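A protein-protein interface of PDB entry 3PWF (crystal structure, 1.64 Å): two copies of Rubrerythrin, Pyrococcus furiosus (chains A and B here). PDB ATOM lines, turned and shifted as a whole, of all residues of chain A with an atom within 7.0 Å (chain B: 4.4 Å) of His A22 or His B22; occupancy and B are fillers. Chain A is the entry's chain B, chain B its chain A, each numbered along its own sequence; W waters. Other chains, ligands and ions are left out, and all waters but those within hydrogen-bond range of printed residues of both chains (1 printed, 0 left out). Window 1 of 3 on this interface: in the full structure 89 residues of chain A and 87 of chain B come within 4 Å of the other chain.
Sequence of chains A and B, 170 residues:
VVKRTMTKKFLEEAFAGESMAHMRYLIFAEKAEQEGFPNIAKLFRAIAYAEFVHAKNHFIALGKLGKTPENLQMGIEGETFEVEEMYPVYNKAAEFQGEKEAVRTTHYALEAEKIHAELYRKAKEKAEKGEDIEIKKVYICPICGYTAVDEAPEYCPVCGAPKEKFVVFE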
ATOM      1  N   ALA A  16       0.062  18.919  -9.354  1.00  0.00           N
ATOM      2  CA  ALA A  16       1.297  19.618  -9.874  1.00  0.00           C
ATOM      3  C   ALA A  16       2.507  19.192  -9.150  1.00  0.00           C
ATOM      4  O   ALA A  16       3.568  18.964  -9.756  1.00  0.00           O
ATOM      5  CB  ALA A  16       1.084  21.167  -9.761  1.00  0.00           C
ATOM      6  N   GLY A  17       2.417  19.106  -7.839  1.00  0.00           N
ATOM      7  CA  GLY A  17       3.623  18.770  -7.045  1.00  0.00           C
ATOM      8  C   GLY A  17       4.106  17.354  -7.340  1.00  0.00           C
ATOM      9  O   GLY A  17       5.332  17.083  -7.420  1.00  0.00           O
ATOM     10  N   GLU A  18       3.161  16.411  -7.420  1.00  0.00           N
ATOM     11  CA  GLU A  18       3.522  15.024  -7.767  1.00  0.00           C
ATOM     12  C   GLU A  18       4.111  14.960  -9.164  1.00  0.00           C
ATOM     13  O   GLU A  18       5.062  14.204  -9.405  1.00  0.00           O
ATOM     14  CB  GLU A  18       2.261  14.099  -7.747  1.00  0.00           C
ATOM     15  CG  GLU A  18       1.768  13.888  -6.324  1.00  0.00           C
ATOM     16  CD  GLU A  18       2.691  12.986  -5.449  1.00  0.00           C
ATOM     17  OE1 GLU A  18       3.627  12.325  -5.901  1.00  0.00           O
ATOM     18  OE2 GLU A  18       2.553  12.939  -4.211  1.00  0.00           O
ATOM     19  N   SER A  19       3.484  15.718 -10.121  1.00  0.00           N
ATOM     20  CA  SER A  19       4.009  15.649 -11.483  1.00  0.00           C
ATOM     21  C   SER A  19       5.493  16.237 -11.515  1.00  0.00           C
ATOM     22  O   SER A  19       6.324  15.651 -12.245  1.00  0.00           O
ATOM     23  CB  SER A  19       3.152  16.531 -12.388  1.00  0.00           C
ATOM     24  OG  SER A  19       1.823  15.952 -12.532  1.00  0.00           O
ATOM     25  N   MET A  20       5.723  17.306 -10.783  1.00  0.00           N
ATOM     26  CA  MET A  20       7.090  17.868 -10.768  1.00  0.00           C
ATOM     27  C   MET A  20       8.056  16.906 -10.083  1.00  0.00           C
ATOM     28  O   MET A  20       9.231  16.806 -10.504  1.00  0.00           O
ATOM     29  CB  MET A  20       7.064  19.288 -10.146  1.00  0.00           C
ATOM     30  CG  MET A  20       6.401  20.201 -11.089  1.00  0.00           C
ATOM     31  SD  MET A  20       6.584  21.980 -10.547  1.00  0.00           S
ATOM     32  CE  MET A  20       5.294  21.919  -9.531  1.00  0.00           C
ATOM     33  N   ALA A  21       7.637  16.277  -8.983  1.00  0.00           N
ATOM     34  CA  ALA A  21       8.554  15.325  -8.296  1.00  0.00           C
ATOM     35  C   ALA A  21       8.905  14.164  -9.242  1.00  0.00           C
ATOM     36  O   ALA A  21      10.033  13.755  -9.370  1.00  0.00           O
ATOM     37  CB  ALA A  21       7.842  14.772  -7.019  1.00  0.00           C
ATOM     38  N   HIS A  22       7.861  13.576  -9.870  1.00  0.00           N
ATOM     39  CA  HIS A  22       8.152  12.550 -10.863  1.00  0.00           C
ATOM     40  C   HIS A  22       9.134  12.993 -11.930  1.00  0.00           C
ATOM     41  O   HIS A  22      10.045  12.225 -12.301  1.00  0.00           O
ATOM     42  CB  HIS A  22       6.762  12.244 -11.554  1.00  0.00           C
ATOM     43  CG  HIS A  22       6.879  11.355 -12.755  1.00  0.00           C
ATOM     44  ND1 HIS A  22       6.769   9.955 -12.739  1.00  0.00           N
ATOM     45  CD2 HIS A  22       7.007  11.706 -14.087  1.00  0.00           C
ATOM     46  CE1 HIS A  22       6.938   9.474 -13.966  1.00  0.00           C
ATOM     47  NE2 HIS A  22       7.059  10.506 -14.820  1.00  0.00           N
ATOM     48  N   MET A  23       8.947  14.190 -12.440  1.00  0.00           N
ATOM     49  CA  MET A  23       9.821  14.697 -13.526  1.00  0.00           C
ATOM     50  C   MET A  23      11.215  14.905 -12.979  1.00  0.00           C
ATOM     51  O   MET A  23      12.156  14.479 -13.673  1.00  0.00           O
ATOM     52  CB  MET A  23       9.236  15.988 -14.065  1.00  0.00           C
ATOM     53  CG  MET A  23       9.954  16.631 -15.295  1.00  0.00           C
ATOM     54  SD  MET A  23      10.070  15.471 -16.670  1.00  0.00           S
ATOM     55  CE  MET A  23       8.335  15.606 -17.233  1.00  0.00           C
ATOM     56  N   ARG A  24      11.356  15.545 -11.819  1.00  0.00           N
ATOM     57  CA  ARG A  24      12.726  15.708 -11.268  1.00  0.00           C
ATOM     58  C   ARG A  24      13.376  14.371 -11.103  1.00  0.00           C
ATOM     59  O   ARG A  24      14.556  14.215 -11.427  1.00  0.00           O
ATOM     60  CB  ARG A  24      12.763  16.425  -9.907  1.00  0.00           C
ATOM     61  CG  ARG A  24      12.298  17.897  -9.995  1.00  0.00           C
ATOM     62  CD  ARG A  24      12.584  18.627  -8.610  1.00  0.00           C
ATOM     63  NE  ARG A  24      11.762  18.133  -7.584  1.00  0.00           N
ATOM     64  CZ  ARG A  24      10.466  18.576  -7.397  1.00  0.00           C
ATOM     65  NH1 ARG A  24       9.792  18.026  -6.442  1.00  0.00           N
ATOM     66  NH2 ARG A  24      10.001  19.619  -8.034  1.00  0.00           N
ATOM     67  N   TYR A  25      12.633  13.354 -10.643  1.00  0.00           N
ATOM     68  CA  TYR A  25      13.243  12.047 -10.419  1.00  0.00           C
ATOM     69  C   TYR A  25      13.682  11.363 -11.722  1.00  0.00           C
ATOM     70  O   TYR A  25      14.723  10.665 -11.763  1.00  0.00           O
ATOM     71  CB  TYR A  25      12.318  11.148  -9.586  1.00  0.00           C
ATOM     72  CG  TYR A  25      12.085  11.716  -8.189  1.00  0.00           C
ATOM     73  CD1 TYR A  25      10.915  11.254  -7.429  1.00  0.00           C
ATOM     74  CD2 TYR A  25      12.954  12.740  -7.612  1.00  0.00           C
ATOM     75  CE1 TYR A  25      10.659  11.818  -6.144  1.00  0.00           C
ATOM     76  CE2 TYR A  25      12.634  13.248  -6.318  1.00  0.00           C
ATOM     77  CZ  TYR A  25      11.530  12.821  -5.655  1.00  0.00           C
ATOM     78  OH  TYR A  25      11.231  13.345  -4.393  1.00  0.00           O
ATOM     79  N   LEU A  26      12.891  11.528 -12.805  1.00  0.00           N
ATOM     80  CA  LEU A  26      13.357  10.970 -14.129  1.00  0.00           C
ATOM     81  C   LEU A  26      14.650  11.762 -14.547  1.00  0.00           C
ATOM     82  O   LEU A  26      15.584  11.096 -15.115  1.00  0.00           O
ATOM     83  CB  LEU A  26      12.301  11.187 -15.207  1.00  0.00           C
ATOM     84  CG  LEU A  26      11.036  10.324 -14.994  1.00  0.00           C
ATOM     85  CD1 LEU A  26      10.164  10.600 -16.285  1.00  0.00           C
ATOM     86  CD2 LEU A  26      11.340   8.744 -14.771  1.00  0.00           C
ATOM     87  N   ILE A  27      14.709  13.046 -14.357  1.00  0.00           N
ATOM     88  CA  ILE A  27      15.931  13.825 -14.736  1.00  0.00           C
ATOM     89  C   ILE A  27      17.109  13.376 -13.831  1.00  0.00           C
ATOM     90  O   ILE A  27      18.220  13.211 -14.372  1.00  0.00           O
ATOM     91  CB  ILE A  27      15.667  15.301 -14.561  1.00  0.00           C
ATOM     92  CG1 ILE A  27      14.508  15.770 -15.506  1.00  0.00           C
ATOM     93  CG2 ILE A  27      16.977  16.201 -14.670  1.00  0.00           C
ATOM     94  CD1 ILE A  27      13.985  17.206 -15.170  1.00  0.00           C
ATOM     95  N   PHE A  28      16.835  13.208 -12.570  1.00  0.00           N
ATOM     96  CA  PHE A  28      17.950  12.708 -11.665  1.00  0.00           C
ATOM     97  C   PHE A  28      18.365  11.271 -11.957  1.00  0.00           C
ATOM     98  O   PHE A  28      19.548  10.979 -11.735  1.00  0.00           O
ATOM     99  CB  PHE A  28      17.463  12.833 -10.222  1.00  0.00           C
ATOM    100  CG  PHE A  28      17.186  14.258  -9.750  1.00  0.00           C
ATOM    101  CD1 PHE A  28      16.430  14.382  -8.546  1.00  0.00           C
ATOM    102  CD2 PHE A  28      17.703  15.399 -10.369  1.00  0.00           C
ATOM    103  CE1 PHE A  28      16.141  15.583  -7.887  1.00  0.00           C
ATOM    104  CE2 PHE A  28      17.390  16.617  -9.747  1.00  0.00           C
ATOM    105  CZ  PHE A  28      16.608  16.746  -8.540  1.00  0.00           C
ATOM    106  N   PHE A  44      15.628   6.162  -8.186  1.00  0.00           N
ATOM    107  CA  PHE A  44      14.885   7.353  -8.706  1.00  0.00           C
ATOM    108  C   PHE A  44      13.798   6.956  -9.714  1.00  0.00           C
ATOM    109  O   PHE A  44      12.707   7.525  -9.644  1.00  0.00           O
ATOM    110  CB  PHE A  44      15.826   8.317  -9.436  1.00  0.00           C
ATOM    111  CG  PHE A  44      16.610   9.297  -8.538  1.00  0.00           C
ATOM    112  CD1 PHE A  44      15.954  10.124  -7.635  1.00  0.00           C
ATOM    113  CD2 PHE A  44      18.047   9.426  -8.666  1.00  0.00           C
ATOM    114  CE1 PHE A  44      16.620  11.043  -6.868  1.00  0.00           C
ATOM    115  CE2 PHE A  44      18.713  10.410  -7.927  1.00  0.00           C
ATOM    116  CZ  PHE A  44      17.980  11.220  -6.998  1.00  0.00           C
ATOM    117  N   ARG A  45      14.031   5.963 -10.566  1.00  0.00           N
ATOM    118  CA  ARG A  45      12.997   5.658 -11.560  1.00  0.00           C
ATOM    119  C   ARG A  45      11.801   4.980 -10.866  1.00  0.00           C
ATOM    120  O   ARG A  45      10.623   5.133 -11.235  1.00  0.00           O
ATOM    121  CB  ARG A  45      13.554   4.732 -12.643  1.00  0.00           C
ATOM    122  CG  ARG A  45      14.499   5.471 -13.524  1.00  0.00           C
ATOM    123  CD  ARG A  45      14.917   4.557 -14.721  1.00  0.00           C
ATOM    124  NE  ARG A  45      15.595   3.372 -14.340  1.00  0.00           N
ATOM    125  CZ  ARG A  45      16.925   3.232 -14.393  1.00  0.00           C
ATOM    126  NH1 ARG A  45      17.707   4.218 -14.850  1.00  0.00           N
ATOM    127  NH2 ARG A  45      17.417   2.118 -14.018  1.00  0.00           N
ATOM    128  N   ILE A  47      10.895   5.349  -7.627  1.00  0.00           N
ATOM    129  CA  ILE A  47      10.101   6.355  -6.846  1.00  0.00           C
ATOM    130  C   ILE A  47       9.355   7.316  -7.841  1.00  0.00           C
ATOM    131  O   ILE A  47       8.208   7.661  -7.549  1.00  0.00           O
ATOM    132  CB  ILE A  47      11.029   7.137  -5.878  1.00  0.00           C
ATOM    133  CG1 ILE A  47      11.409   6.097  -4.791  1.00  0.00           C
ATOM    134  CG2 ILE A  47      10.238   8.310  -5.208  1.00  0.00           C
ATOM    135  CD1 ILE A  47      12.489   6.617  -3.726  1.00  0.00           C
ATOM    136  N   ALA A  48       9.940   7.586  -9.021  1.00  0.00           N
ATOM    137  CA  ALA A  48       9.144   8.371 -10.014  1.00  0.00           C
ATOM    138  C   ALA A  48       7.861   7.618 -10.324  1.00  0.00           C
ATOM    139  O   ALA A  48       6.810   8.311 -10.519  1.00  0.00           O
ATOM    140  CB  ALA A  48       9.952   8.500 -11.309  1.00  0.00           C
ATOM    141  N   TYR A  49       7.855   6.271 -10.463  1.00  0.00           N
ATOM    142  CA  TYR A  49       6.579   5.577 -10.726  1.00  0.00           C
ATOM    143  C   TYR A  49       5.645   5.730  -9.510  1.00  0.00           C
ATOM    144  O   TYR A  49       4.423   5.854  -9.694  1.00  0.00           O
ATOM    145  CB  TYR A  49       6.905   4.083 -11.035  1.00  0.00           C
ATOM    146  CG  TYR A  49       5.635   3.335 -11.344  1.00  0.00           C
ATOM    147  CD1 TYR A  49       4.983   3.506 -12.485  1.00  0.00           C
ATOM    148  CD2 TYR A  49       5.068   2.548 -10.347  1.00  0.00           C
ATOM    149  CE1 TYR A  49       3.698   2.807 -12.685  1.00  0.00           C
ATOM    150  CE2 TYR A  49       3.876   1.930 -10.525  1.00  0.00           C
ATOM    151  CZ  TYR A  49       3.229   2.103 -11.627  1.00  0.00           C
ATOM    152  OH  TYR A  49       2.034   1.367 -11.582  1.00  0.00           O
ATOM    153  N   ALA A  50       6.121   5.676  -8.287  1.00  0.00           N
ATOM    154  CA  ALA A  50       5.235   5.855  -7.140  1.00  0.00           C
ATOM    155  C   ALA A  50       4.595   7.256  -7.216  1.00  0.00           C
ATOM    156  O   ALA A  50       3.445   7.399  -6.808  1.00  0.00           O
ATOM    157  CB  ALA A  50       6.101   5.790  -5.849  1.00  0.00           C
ATOM    158  N   GLU A  51       5.330   8.281  -7.705  1.00  0.00           N
ATOM    159  CA  GLU A  51       4.674   9.635  -7.784  1.00  0.00           C
ATOM    160  C   GLU A  51       3.658   9.681  -8.922  1.00  0.00           C
ATOM    161  O   GLU A  51       2.715  10.439  -8.854  1.00  0.00           O
ATOM    162  CB  GLU A  51       5.751  10.731  -8.028  1.00  0.00           C
ATOM    163  CG  GLU A  51       7.018  10.630  -7.072  1.00  0.00           C
ATOM    164  CD  GLU A  51       6.729  10.619  -5.540  1.00  0.00           C
ATOM    165  OE1 GLU A  51       5.583  10.441  -5.111  1.00  0.00           O
ATOM    166  OE2 GLU A  51       7.744  10.790  -4.767  1.00  0.00           O
ATOM    167  N   PHE A  52       3.904   8.887  -9.994  1.00  0.00           N
ATOM    168  CA  PHE A  52       2.842   8.697 -11.035  1.00  0.00           C
ATOM    169  C   PHE A  52       1.597   8.106 -10.385  1.00  0.00           C
ATOM    170  O   PHE A  52       0.500   8.518 -10.688  1.00  0.00           O
ATOM    171  CB  PHE A  52       3.407   7.799 -12.183  1.00  0.00           C
ATOM    172  CG  PHE A  52       2.297   7.105 -12.960  1.00  0.00           C
ATOM    173  CD1 PHE A  52       1.771   7.699 -14.042  1.00  0.00           C
ATOM    174  CD2 PHE A  52       1.895   5.829 -12.540  1.00  0.00           C
ATOM    175  CE1 PHE A  52       0.689   7.069 -14.752  1.00  0.00           C
ATOM    176  CE2 PHE A  52       0.794   5.156 -13.245  1.00  0.00           C
ATOM    177  CZ  PHE A  52       0.248   5.779 -14.323  1.00  0.00           C
ATOM    178  N   VAL A  53       1.728   7.084  -9.549  1.00  0.00           N
ATOM    179  CA  VAL A  53       0.595   6.579  -8.875  1.00  0.00           C
ATOM    180  C   VAL A  53      -0.132   7.673  -8.044  1.00  0.00           C
ATOM    181  O   VAL A  53      -1.362   7.801  -8.130  1.00  0.00           O
ATOM    182  CB  VAL A  53       0.916   5.397  -7.936  1.00  0.00           C
ATOM    183  CG1 VAL A  53      -0.249   4.923  -7.095  1.00  0.00           C
ATOM    184  CG2 VAL A  53       1.534   4.191  -8.753  1.00  0.00           C
ATOM    185  N   ALA A  55      -0.062  10.943  -8.421  1.00  0.00           N
ATOM    186  CA  ALA A  55      -0.633  11.991  -9.297  1.00  0.00           C
ATOM    187  C   ALA A  55      -1.888  11.412  -9.953  1.00  0.00           C
ATOM    188  O   ALA A  55      -2.893  12.141  -9.999  1.00  0.00           O
ATOM    189  CB  ALA A  55       0.423  12.362 -10.355  1.00  0.00           C
ATOM    190  N   GLU B  18       4.969  21.425 -18.277  1.00  0.00           N
ATOM    191  CA  GLU B  18       5.526  20.282 -19.018  1.00  0.00           C
ATOM    192  C   GLU B  18       5.378  19.065 -18.160  1.00  0.00           C
ATOM    193  O   GLU B  18       5.123  17.935 -18.675  1.00  0.00           O
ATOM    194  CB  GLU B  18       7.021  20.502 -19.326  1.00  0.00           C
ATOM    195  CG  GLU B  18       7.243  21.633 -20.409  1.00  0.00           C
ATOM    196  CD  GLU B  18       6.753  21.146 -21.835  1.00  0.00           C
ATOM    197  OE1 GLU B  18       6.659  21.952 -22.771  1.00  0.00           O
ATOM    198  OE2 GLU B  18       6.529  19.956 -22.078  1.00  0.00           O
ATOM    199  N   SER B  19       5.728  19.211 -16.854  1.00  0.00           N
ATOM    200  CA  SER B  19       5.593  18.058 -15.929  1.00  0.00           C
ATOM    201  C   SER B  19       4.121  17.574 -15.908  1.00  0.00           C
ATOM    202  O   SER B  19       3.928  16.320 -15.927  1.00  0.00           O
ATOM    203  CB  SER B  19       5.943  18.512 -14.504  1.00  0.00           C
ATOM    204  OG  SER B  19       7.430  18.778 -14.521  1.00  0.00           O
ATOM    205  N   MET B  20       3.177  18.486 -15.848  1.00  0.00           N
ATOM    206  CA  MET B  20       1.764  18.013 -15.794  1.00  0.00           C
ATOM    207  C   MET B  20       1.327  17.413 -17.158  1.00  0.00           C
ATOM    208  O   MET B  20       0.565  16.391 -17.152  1.00  0.00           O
ATOM    209  CB  MET B  20       0.791  19.133 -15.361  1.00  0.00           C
ATOM    210  CG  MET B  20       1.064  19.423 -13.925  1.00  0.00           C
ATOM    211  SD  MET B  20      -0.143  20.645 -13.290  1.00  0.00           S
ATOM    212  CE  MET B  20       0.600  22.022 -13.888  1.00  0.00           C
ATOM    213  N   ALA B  21       1.834  17.970 -18.290  1.00  0.00           N
ATOM    214  CA  ALA B  21       1.497  17.324 -19.531  1.00  0.00           C
ATOM    215  C   ALA B  21       2.049  15.948 -19.721  1.00  0.00           C
ATOM    216  O   ALA B  21       1.371  15.003 -20.057  1.00  0.00           O
ATOM    217  CB  ALA B  21       1.993  18.249 -20.708  1.00  0.00           C
ATOM    218  N   HIS B  22       3.299  15.741 -19.327  1.00  0.00           N
ATOM    219  CA  HIS B  22       3.877  14.434 -19.324  1.00  0.00           C
ATOM    220  C   HIS B  22       3.088  13.478 -18.452  1.00  0.00           C
ATOM    221  O   HIS B  22       2.842  12.335 -18.872  1.00  0.00           O
ATOM    222  CB  HIS B  22       5.339  14.603 -18.728  1.00  0.00           C
ATOM    223  CG  HIS B  22       5.990  13.308 -18.362  1.00  0.00           C
ATOM    224  ND1 HIS B  22       6.804  12.596 -19.242  1.00  0.00           N
ATOM    225  CD2 HIS B  22       5.998  12.590 -17.196  1.00  0.00           C
ATOM    226  CE1 HIS B  22       7.265  11.485 -18.637  1.00  0.00           C
ATOM    227  NE2 HIS B  22       6.786  11.471 -17.403  1.00  0.00           N
ATOM    228  N   MET B  23       2.673  13.883 -17.234  1.00  0.00           N
ATOM    229  CA  MET B  23       1.934  13.012 -16.299  1.00  0.00           C
ATOM    230  C   MET B  23       0.565  12.676 -16.917  1.00  0.00           C
ATOM    231  O   MET B  23       0.202  11.513 -16.887  1.00  0.00           O
ATOM    232  CB  MET B  23       1.843  13.785 -15.058  1.00  0.00           C
ATOM    233  CG  MET B  23       1.163  12.953 -13.876  1.00  0.00           C
ATOM    234  SD  MET B  23       2.007  11.336 -13.587  1.00  0.00           S
ATOM    235  CE  MET B  23       3.470  11.981 -12.720  1.00  0.00           C
ATOM    236  N   ARG B  24      -0.105  13.674 -17.469  1.00  0.00           N
ATOM    237  CA  ARG B  24      -1.434  13.394 -18.105  1.00  0.00           C
ATOM    238  C   ARG B  24      -1.224  12.363 -19.194  1.00  0.00           C
ATOM    239  O   ARG B  24      -2.078  11.432 -19.302  1.00  0.00           O
ATOM    240  CB  ARG B  24      -2.097  14.660 -18.692  1.00  0.00           C
ATOM    241  CG  ARG B  24      -2.565  15.575 -17.558  1.00  0.00           C
ATOM    242  CD  ARG B  24      -3.574  16.671 -18.131  1.00  0.00           C
ATOM    243  NE  ARG B  24      -2.845  17.561 -18.979  1.00  0.00           N
ATOM    244  CZ  ARG B  24      -2.132  18.640 -18.552  1.00  0.00           C
ATOM    245  NH1 ARG B  24      -1.473  19.319 -19.457  1.00  0.00           N
ATOM    246  NH2 ARG B  24      -2.226  19.092 -17.342  1.00  0.00           N
ATOM    247  N   TYR B  25      -0.177  12.474 -20.023  1.00  0.00           N
ATOM    248  CA  TYR B  25      -0.062  11.593 -21.148  1.00  0.00           C
ATOM    249  C   TYR B  25       0.287  10.227 -20.694  1.00  0.00           C
ATOM    250  O   TYR B  25      -0.131   9.274 -21.351  1.00  0.00           O
ATOM    251  CB  TYR B  25       1.016  12.155 -22.154  1.00  0.00           C
ATOM    252  CG  TYR B  25       0.558  13.505 -22.694  1.00  0.00           C
ATOM    253  CD1 TYR B  25       1.524  14.345 -23.319  1.00  0.00           C
ATOM    254  CD2 TYR B  25      -0.801  13.916 -22.721  1.00  0.00           C
ATOM    255  CE1 TYR B  25       1.165  15.612 -23.824  1.00  0.00           C
ATOM    256  CE2 TYR B  25      -1.122  15.198 -23.215  1.00  0.00           C
ATOM    257  CZ  TYR B  25      -0.160  16.007 -23.775  1.00  0.00           C
ATOM    258  OH  TYR B  25      -0.496  17.283 -24.292  1.00  0.00           O
ATOM    259  N   LEU B  26       1.083  10.059 -19.598  1.00  0.00           N
ATOM    260  CA  LEU B  26       1.267   8.683 -19.053  1.00  0.00           C
ATOM    261  C   LEU B  26      -0.069   8.090 -18.562  1.00  0.00           C
ATOM    262  O   LEU B  26      -0.254   6.886 -18.745  1.00  0.00           O
ATOM    263  CB  LEU B  26       2.243   8.653 -17.864  1.00  0.00           C
ATOM    264  CG  LEU B  26       3.667   8.982 -18.306  1.00  0.00           C
ATOM    265  CD1 LEU B  26       4.531   8.915 -16.995  1.00  0.00           C
ATOM    266  CD2 LEU B  26       4.250   8.075 -19.277  1.00  0.00           C
ATOM    267  N   ALA B  48       4.839  11.847 -24.226  1.00  0.00           N
ATOM    268  CA  ALA B  48       5.274  12.097 -22.813  1.00  0.00           C
ATOM    269  C   ALA B  48       6.784  12.233 -22.755  1.00  0.00           C
ATOM    270  O   ALA B  48       7.293  13.028 -21.949  1.00  0.00           O
ATOM    271  CB  ALA B  48       4.765  10.952 -21.847  1.00  0.00           C
ATOM    272  N   GLU B  51       7.800  15.623 -23.697  1.00  0.00           N
ATOM    273  CA  GLU B  51       7.575  16.682 -22.656  1.00  0.00           C
ATOM    274  C   GLU B  51       8.598  16.534 -21.532  1.00  0.00           C
ATOM    275  O   GLU B  51       8.978  17.546 -20.933  1.00  0.00           O
ATOM    276  CB  GLU B  51       6.181  16.519 -22.014  1.00  0.00           C
ATOM    277  CG  GLU B  51       4.993  16.331 -23.102  1.00  0.00           C
ATOM    278  CD  GLU B  51       4.898  17.527 -24.149  1.00  0.00           C
ATOM    279  OE1 GLU B  51       3.782  17.520 -24.823  1.00  0.00           O
ATOM    280  OE2 GLU B  51       5.820  18.379 -24.311  1.00  0.00           O
ATOM    281  N   PHE B  52       9.125  15.315 -21.277  1.00  0.00           N
ATOM    282  CA  PHE B  52      10.299  15.170 -20.375  1.00  0.00           C
ATOM    283  C   PHE B  52      11.463  15.926 -20.954  1.00  0.00           C
ATOM    284  O   PHE B  52      12.179  16.587 -20.190  1.00  0.00           O
ATOM    285  CB  PHE B  52      10.608  13.660 -20.269  1.00  0.00           C
ATOM    286  CG  PHE B  52      12.069  13.383 -19.812  1.00  0.00           C
ATOM    287  CD1 PHE B  52      12.428  13.383 -18.472  1.00  0.00           C
ATOM    288  CD2 PHE B  52      13.012  13.169 -20.793  1.00  0.00           C
ATOM    289  CE1 PHE B  52      13.802  13.164 -18.063  1.00  0.00           C
ATOM    290  CE2 PHE B  52      14.397  12.949 -20.393  1.00  0.00           C
ATOM    291  CZ  PHE B  52      14.759  12.981 -19.020  1.00  0.00           C
HETATM  292  O   HOH W   1       5.644  14.517 -14.682  1.00  0.00           O
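NE2 of His A22 lies within hydrogen-bond range of NE2 of His B22 (2.8 Å).
A ring nitrogen (ND1) of His A22 lies within hydrogen-bond range of the backbone carbonyl oxygen (O) of Ala A48 (2.8 Å). A ring nitrogen (ND1) of His B22 sits at hydrogen-bond distance from the backbone carbonyl oxygen of Ala B48 (2.8 Å).
Among the printed residues, merely in contact across the chains: Ser A19 with Met B23, Met A23 with Ser B19, His A22 with Met B23, Met A23 with His B22, Met A23 with Phe B52, Ser A19 with Ser B19, Ala A55 with Met B23, Leu A26 with His B22, Phe A52 with Met B23, His A22 with Leu B26, Ile A27 with Phe B52, Ala A16 with Met B20, Leu A26 with Phe B52, Ser A19 with Met B20, Phe A52 with Leu B26 and Met A20 with Ser B19.
His A22 touches just these residues of chain B: His B22, Met B23 and Leu B26. Printed residues of chain A within 4 Å of His B22: His A22 (2.8 Å), Met A23 (3.5 Å) and Leu A26 (3.7 Å). Of the printed residues of chain A, Leu B26 touches His A22 (3.7 Å) and Phe A52 (3.8 Å). Of the printed residues of chain B, Leu A26 touches His B22 (3.7 Å) and Phe B52 (3.8 Å). Of the printed residues of chain A, Phe B52 touches Met A23 (3.6 Å), Leu A26 (3.8 Å) and Ile A27 (3.7 Å). Printed residues of chain B within 4 Å of Phe A52: Met B23 (3.7 Å) and Leu B26 (3.8 Å). Ala B48 touches none of the printed residues of chain A. The nearest printed residue of chain B that does not touch His A22 is Ser B19 (5.8 Å).
Hydrophobic or aromatic side chains of chain B within 4 Å of the printed part of chain A: Met B20, His B22, Met B23, Leu B26 and Phe B52. Among the printed residues, 17 pairs touch across the chains.
Ser A19 touches Met B23, and with the chains exchanged Met A23 touches Ser B19. His A22 touches Met B23, and with the chains exchanged Met A23 touches His B22. Met A23 touches Phe B52, and with the chains exchanged Phe A52 touches Met B23. Leu A26 touches Phe B52, and with the chains exchanged Phe A52 touches Leu B26. 12 positions are printed for both chains.
Water W1 lies within hydrogen-bond range of the backbone carbonyl oxygen of Ser A19 (2.8 Å) and the backbone carbonyl oxygen of Ser B19 (2.8 Å).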
